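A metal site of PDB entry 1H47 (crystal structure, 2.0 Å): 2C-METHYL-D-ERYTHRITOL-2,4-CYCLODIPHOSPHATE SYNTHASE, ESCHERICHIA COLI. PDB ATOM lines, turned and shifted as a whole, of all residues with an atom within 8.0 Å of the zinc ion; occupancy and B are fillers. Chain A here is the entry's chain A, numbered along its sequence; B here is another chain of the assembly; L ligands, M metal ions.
A ring nitrogen (ND1) of His 44 is bound to the zinc ion, 2.0 Å away.
The zinc ion is bound by the side-chain carboxylate (OD2) of Asp 10, at 2.1 Å.
NE2 of His 12 is bound to the zinc ion (2.2 Å).
Slightly farther from the zinc ion lies OD1 of Asp 10 (2.8 Å).
A ring nitrogen (NE2) of His 44 sits at hydrogen-bond distance from the side-chain hydroxyl (OG) of Ser 75 (2.8 Å).
OE1 of Glu 137 of chain B lies within hydrogen-bond range of ND1 of His 12 (2.8 Å).
ND1 of His 12 lies within hydrogen-bond range of O of Leu 34, at 3.3 Å.
The side-chain hydroxyl (OG1) of Thr 134 of chain B is in hydrogen-bond range of an oxygen (O1) of the ligand (3.3 Å).
The backbone NH of Thr 135 of chain B is in hydrogen-bond range of an oxygen (O1) of the ligand, at 2.9 Å.
The side-chain hydroxyl of Thr 135 of chain B is in hydrogen-bond range of an oxygen (O1) of the ligand, at 2.7 Å.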
ATOM      1  N   PHE A   9       4.372  19.138  26.074  1.00  0.00           N
ATOM      2  CA  PHE A   9       5.283  19.269  24.965  1.00  0.00           C
ATOM      3  C   PHE A   9       4.972  20.568  24.206  1.00  0.00           C
ATOM      4  O   PHE A   9       3.825  20.915  24.027  1.00  0.00           O
ATOM      5  CB  PHE A   9       5.190  18.041  24.052  1.00  0.00           C
ATOM      6  CG  PHE A   9       6.064  18.156  22.800  1.00  0.00           C
ATOM      7  CD1 PHE A   9       7.422  18.003  22.878  1.00  0.00           C
ATOM      8  CD2 PHE A   9       5.510  18.418  21.559  1.00  0.00           C
ATOM      9  CE1 PHE A   9       8.236  18.091  21.732  1.00  0.00           C
ATOM     10  CE2 PHE A   9       6.329  18.512  20.395  1.00  0.00           C
ATOM     11  CZ  PHE A   9       7.681  18.338  20.508  1.00  0.00           C
ATOM     12  N   ASP A  10       6.001  21.298  23.798  1.00  0.00           N
ATOM     13  CA  ASP A  10       5.792  22.549  23.056  1.00  0.00           C
ATOM     14  C   ASP A  10       6.904  22.769  22.026  1.00  0.00           C
ATOM     15  O   ASP A  10       7.999  22.255  22.156  1.00  0.00           O
ATOM     16  CB  ASP A  10       5.778  23.720  24.012  1.00  0.00           C
ATOM     17  CG  ASP A  10       5.145  24.951  23.435  1.00  0.00           C
ATOM     18  OD1 ASP A  10       4.255  24.888  22.589  1.00  0.00           O
ATOM     19  OD2 ASP A  10       5.534  26.063  23.770  1.00  0.00           O
ATOM     20  N   VAL A  11       6.595  23.550  21.011  1.00  0.00           N
ATOM     21  CA  VAL A  11       7.584  23.911  19.990  1.00  0.00           C
ATOM     22  C   VAL A  11       7.377  25.365  19.666  1.00  0.00           C
ATOM     23  O   VAL A  11       6.245  25.812  19.536  1.00  0.00           O
ATOM     24  CB  VAL A  11       7.403  23.095  18.733  1.00  0.00           C
ATOM     25  CG1 VAL A  11       8.359  23.590  17.577  1.00  0.00           C
ATOM     26  CG2 VAL A  11       7.651  21.684  19.028  1.00  0.00           C
ATOM     27  N   HIS A  12       8.473  26.106  19.581  1.00  0.00           N
ATOM     28  CA  HIS A  12       8.435  27.390  18.923  1.00  0.00           C
ATOM     29  C   HIS A  12       9.484  27.536  17.808  1.00  0.00           C
ATOM     30  O   HIS A  12      10.635  27.136  17.947  1.00  0.00           O
ATOM     31  CB  HIS A  12       8.510  28.535  19.922  1.00  0.00           C
ATOM     32  CG  HIS A  12       7.202  28.741  20.632  1.00  0.00           C
ATOM     33  ND1 HIS A  12       6.132  29.383  20.054  1.00  0.00           N
ATOM     34  CD2 HIS A  12       6.778  28.283  21.849  1.00  0.00           C
ATOM     35  CE1 HIS A  12       5.108  29.352  20.900  1.00  0.00           C
ATOM     36  NE2 HIS A  12       5.473  28.687  21.989  1.00  0.00           N
ATOM     37  N   LEU A  34       9.270  33.324  17.598  1.00  0.00           N
ATOM     38  CA  LEU A  34       7.959  33.782  17.170  1.00  0.00           C
ATOM     39  C   LEU A  34       6.867  33.110  17.973  1.00  0.00           C
ATOM     40  O   LEU A  34       6.845  31.885  18.096  1.00  0.00           O
ATOM     41  CB  LEU A  34       7.690  33.427  15.706  1.00  0.00           C
ATOM     42  CG  LEU A  34       8.570  34.053  14.621  1.00  0.00           C
ATOM     43  CD1 LEU A  34       7.875  33.943  13.262  1.00  0.00           C
ATOM     44  CD2 LEU A  34       8.925  35.519  14.930  1.00  0.00           C
ATOM     45  N   ALA A  35       5.943  33.921  18.473  1.00  0.00           N
ATOM     46  CA  ALA A  35       4.719  33.407  19.094  1.00  0.00           C
ATOM     47  C   ALA A  35       3.662  34.494  19.258  1.00  0.00           C
ATOM     48  O   ALA A  35       3.970  35.682  19.416  1.00  0.00           O
ATOM     49  CB  ALA A  35       5.039  32.779  20.435  1.00  0.00           C
ATOM     50  N   HIS A  36       2.400  34.055  19.192  1.00  0.00           N
ATOM     51  CA  HIS A  36       1.289  34.801  19.789  1.00  0.00           C
ATOM     52  C   HIS A  36       1.724  35.326  21.144  1.00  0.00           C
ATOM     53  O   HIS A  36       1.374  36.457  21.520  1.00  0.00           O
ATOM     54  CB  HIS A  36       0.070  33.893  19.982  1.00  0.00           C
ATOM     55  N   SER A  37       2.515  34.515  21.849  1.00  0.00           N
ATOM     56  CA  SER A  37       2.993  34.758  23.214  1.00  0.00           C
ATOM     57  C   SER A  37       4.486  35.100  23.235  1.00  0.00           C
ATOM     58  O   SER A  37       5.029  35.520  22.218  1.00  0.00           O
ATOM     59  CB  SER A  37       2.724  33.484  24.021  1.00  0.00           C
ATOM     60  OG  SER A  37       3.307  32.349  23.384  1.00  0.00           O
ATOM     61  N   ASP A  38       5.165  34.950  24.370  1.00  0.00           N
ATOM     62  CA  ASP A  38       6.621  35.183  24.388  1.00  0.00           C
ATOM     63  C   ASP A  38       7.477  33.994  23.915  1.00  0.00           C
ATOM     64  O   ASP A  38       8.693  34.116  23.892  1.00  0.00           O
ATOM     65  CB  ASP A  38       7.099  35.658  25.780  1.00  0.00           C
ATOM     66  CG  ASP A  38       6.997  34.583  26.857  1.00  0.00           C
ATOM     67  OD1 ASP A  38       6.523  33.465  26.522  1.00  0.00           O
ATOM     68  OD2 ASP A  38       7.343  34.797  28.052  1.00  0.00           O
ATOM     69  N   GLY A  39       6.875  32.862  23.556  1.00  0.00           N
ATOM     70  CA  GLY A  39       7.615  31.747  22.951  1.00  0.00           C
ATOM     71  C   GLY A  39       8.436  30.920  23.949  1.00  0.00           C
ATOM     72  O   GLY A  39       9.350  30.154  23.550  1.00  0.00           O
ATOM     73  N   ASP A  40       8.106  31.037  25.246  1.00  0.00           N
ATOM     74  CA  ASP A  40       8.810  30.292  26.278  1.00  0.00           C
ATOM     75  C   ASP A  40       8.408  28.817  26.226  1.00  0.00           C
ATOM     76  O   ASP A  40       7.488  28.386  26.947  1.00  0.00           O
ATOM     77  CB  ASP A  40       8.535  30.887  27.645  1.00  0.00           C
ATOM     78  CG  ASP A  40       9.503  30.423  28.684  1.00  0.00           C
ATOM     79  OD1 ASP A  40       9.987  29.232  28.611  1.00  0.00           O
ATOM     80  OD2 ASP A  40       9.857  31.165  29.619  1.00  0.00           O
ATOM     81  N   VAL A  41       9.090  28.029  25.386  1.00  0.00           N
ATOM     82  CA  VAL A  41       8.705  26.630  25.191  1.00  0.00           C
ATOM     83  C   VAL A  41       8.748  25.838  26.443  1.00  0.00           C
ATOM     84  O   VAL A  41       7.966  24.937  26.578  1.00  0.00           O
ATOM     85  CB  VAL A  41       9.564  25.786  24.209  1.00  0.00           C
ATOM     86  CG1 VAL A  41       9.046  25.961  22.817  1.00  0.00           C
ATOM     87  CG2 VAL A  41      11.056  26.062  24.315  1.00  0.00           C
ATOM     88  N   ALA A  42       9.730  26.119  27.277  1.00  0.00           N
ATOM     89  CA  ALA A  42       9.920  25.386  28.530  1.00  0.00           C
ATOM     90  C   ALA A  42       8.774  25.608  29.533  1.00  0.00           C
ATOM     91  O   ALA A  42       8.262  24.654  30.113  1.00  0.00           O
ATOM     92  CB  ALA A  42      11.248  25.778  29.170  1.00  0.00           C
ATOM     93  N   LEU A  43       8.428  26.865  29.769  1.00  0.00           N
ATOM     94  CA  LEU A  43       7.311  27.177  30.680  1.00  0.00           C
ATOM     95  C   LEU A  43       5.990  26.759  30.142  1.00  0.00           C
ATOM     96  O   LEU A  43       5.134  26.316  30.906  1.00  0.00           O
ATOM     97  CB  LEU A  43       7.330  28.648  31.129  1.00  0.00           C
ATOM     98  CG  LEU A  43       8.636  29.062  31.858  1.00  0.00           C
ATOM     99  CD1 LEU A  43       8.555  30.505  32.371  1.00  0.00           C
ATOM    100  CD2 LEU A  43       8.958  28.128  33.050  1.00  0.00           C
ATOM    101  N   HIS A  44       5.826  26.773  28.808  1.00  0.00           N
ATOM    102  CA  HIS A  44       4.609  26.278  28.202  1.00  0.00           C
ATOM    103  C   HIS A  44       4.479  24.768  28.407  1.00  0.00           C
ATOM    104  O   HIS A  44       3.416  24.292  28.798  1.00  0.00           O
ATOM    105  CB  HIS A  44       4.535  26.611  26.719  1.00  0.00           C
ATOM    106  CG  HIS A  44       4.368  28.067  26.437  1.00  0.00           C
ATOM    107  ND1 HIS A  44       4.253  28.572  25.155  1.00  0.00           N
ATOM    108  CD2 HIS A  44       4.278  29.139  27.265  1.00  0.00           C
ATOM    109  CE1 HIS A  44       4.114  29.881  25.208  1.00  0.00           C
ATOM    110  NE2 HIS A  44       4.150  30.257  26.474  1.00  0.00           N
ATOM    111  N   ALA A  45       5.538  24.035  28.139  1.00  0.00           N
ATOM    112  CA  ALA A  45       5.451  22.592  28.226  1.00  0.00           C
ATOM    113  C   ALA A  45       5.222  22.239  29.697  1.00  0.00           C
ATOM    114  O   ALA A  45       4.483  21.355  30.021  1.00  0.00           O
ATOM    115  CB  ALA A  45       6.711  21.942  27.697  1.00  0.00           C
ATOM    116  N   ASP A  48       1.541  22.891  30.661  1.00  0.00           N
ATOM    117  CA  ASP A  48       0.688  21.826  30.192  1.00  0.00           C
ATOM    118  C   ASP A  48       0.825  20.543  31.046  1.00  0.00           C
ATOM    119  O   ASP A  48      -0.155  19.825  31.188  1.00  0.00           O
ATOM    120  CB  ASP A  48       0.988  21.473  28.730  1.00  0.00           C
ATOM    121  CG  ASP A  48       0.208  22.315  27.725  1.00  0.00           C
ATOM    122  OD1 ASP A  48      -0.659  23.122  28.150  1.00  0.00           O
ATOM    123  OD2 ASP A  48       0.364  22.224  26.484  1.00  0.00           O
ATOM    124  N   ILE A  59      -2.891  24.846  28.273  1.00  0.00           N
ATOM    125  CA  ILE A  59      -2.763  26.308  28.246  1.00  0.00           C
ATOM    126  C   ILE A  59      -3.753  26.997  27.312  1.00  0.00           C
ATOM    127  O   ILE A  59      -4.329  28.015  27.672  1.00  0.00           O
ATOM    128  CB  ILE A  59      -1.342  26.812  27.862  1.00  0.00           C
ATOM    129  CG1 ILE A  59      -0.624  25.850  26.904  1.00  0.00           C
ATOM    130  CG2 ILE A  59      -0.566  27.084  29.079  1.00  0.00           C
ATOM    131  CD1 ILE A  59       0.365  26.505  25.963  1.00  0.00           C
ATOM    132  N   SER A  75       4.859  34.141  30.043  1.00  0.00           N
ATOM    133  CA  SER A  75       4.687  32.735  30.372  1.00  0.00           C
ATOM    134  C   SER A  75       4.763  32.477  31.860  1.00  0.00           C
ATOM    135  O   SER A  75       4.173  31.520  32.313  1.00  0.00           O
ATOM    136  CB  SER A  75       5.710  31.895  29.614  1.00  0.00           C
ATOM    137  OG  SER A  75       5.444  32.025  28.210  1.00  0.00           O
ATOM    138  N   THR B 134      -1.210  20.006  20.972  1.00  0.00           N
ATOM    139  CA  THR B 134      -0.346  21.123  20.617  1.00  0.00           C
ATOM    140  C   THR B 134       0.016  20.993  19.128  1.00  0.00           C
ATOM    141  O   THR B 134       0.005  19.888  18.580  1.00  0.00           O
ATOM    142  CB  THR B 134       0.892  21.156  21.512  1.00  0.00           C
ATOM    143  OG1 THR B 134       1.725  22.280  21.217  1.00  0.00           O
ATOM    144  CG2 THR B 134       1.794  19.951  21.315  1.00  0.00           C
ATOM    145  N   THR B 135       0.298  22.127  18.492  1.00  0.00           N
ATOM    146  CA  THR B 135       0.911  22.120  17.170  1.00  0.00           C
ATOM    147  C   THR B 135       2.414  22.159  17.358  1.00  0.00           C
ATOM    148  O   THR B 135       2.895  22.263  18.481  1.00  0.00           O
ATOM    149  CB  THR B 135       0.523  23.349  16.335  1.00  0.00           C
ATOM    150  OG1 THR B 135       1.228  24.497  16.799  1.00  0.00           O
ATOM    151  CG2 THR B 135      -0.931  23.721  16.495  1.00  0.00           C
ATOM    152  N   GLU B 137       3.989  24.502  15.383  1.00  0.00           N
ATOM    153  CA  GLU B 137       4.218  25.805  14.783  1.00  0.00           C
ATOM    154  C   GLU B 137       4.735  25.634  13.348  1.00  0.00           C
ATOM    155  O   GLU B 137       5.765  26.210  12.985  1.00  0.00           O
ATOM    156  CB  GLU B 137       5.265  26.531  15.613  1.00  0.00           C
ATOM    157  CG  GLU B 137       5.144  28.015  15.645  1.00  0.00           C
ATOM    158  CD  GLU B 137       5.362  28.563  17.055  1.00  0.00           C
ATOM    159  OE1 GLU B 137       6.378  29.306  17.224  1.00  0.00           O
ATOM    160  OE2 GLU B 137       4.507  28.257  17.953  1.00  0.00           O
HETATM  161  O1  LIG L   1       0.699  24.836  19.405  1.00  0.00           O
HETATM  162  P1  LIG L   1      -0.227  26.006  19.942  1.00  0.00           P
HETATM  163  O2  LIG L   1       0.278  26.601  21.328  1.00  0.00           O
HETATM  164  O3  LIG L   1      -0.285  27.234  18.946  1.00  0.00           O
HETATM  165  O4  LIG L   1      -1.635  25.370  20.186  1.00  0.00           O
HETATM  166  C1  LIG L   1      -2.573  26.327  20.614  1.00  0.00           C
HETATM  167  C2  LIG L   1      -3.676  25.646  21.357  1.00  0.00           C
HETATM  168  O5  LIG L   1      -4.676  25.099  20.480  1.00  0.00           O
HETATM  169  C3  LIG L   1      -3.287  24.574  22.376  1.00  0.00           C
HETATM  170  O6  LIG L   1      -2.986  24.961  23.718  1.00  0.00           O
HETATM  171  C4  LIG L   1      -4.380  23.562  22.183  1.00  0.00           C
HETATM  172  O7  LIG L   1      -5.260  23.997  23.203  1.00  0.00           O
HETATM  173  C5  LIG L   1      -5.152  23.839  20.908  1.00  0.00           C
HETATM  174  N1  LIG L   1      -4.863  22.886  19.800  1.00  0.00           N
HETATM  175  C6  LIG L   1      -5.909  22.111  19.310  1.00  0.00           C
HETATM  176  N2  LIG L   1      -5.731  21.239  18.291  1.00  0.00           N
HETATM  177  C7  LIG L   1      -4.527  21.089  17.695  1.00  0.00           C
HETATM  178  C8  LIG L   1      -3.443  21.869  18.130  1.00  0.00           C
HETATM  179  C9  LIG L   1      -3.643  22.749  19.212  1.00  0.00           C
HETATM  180  O8  LIG L   1      -7.013  22.190  19.850  1.00  0.00           O
HETATM  181  N3  LIG L   1      -4.432  20.198  16.682  1.00  0.00           N
HETATM  182 ZN    ZN M   1       4.155  27.608  23.379  1.00  0.00          ZN
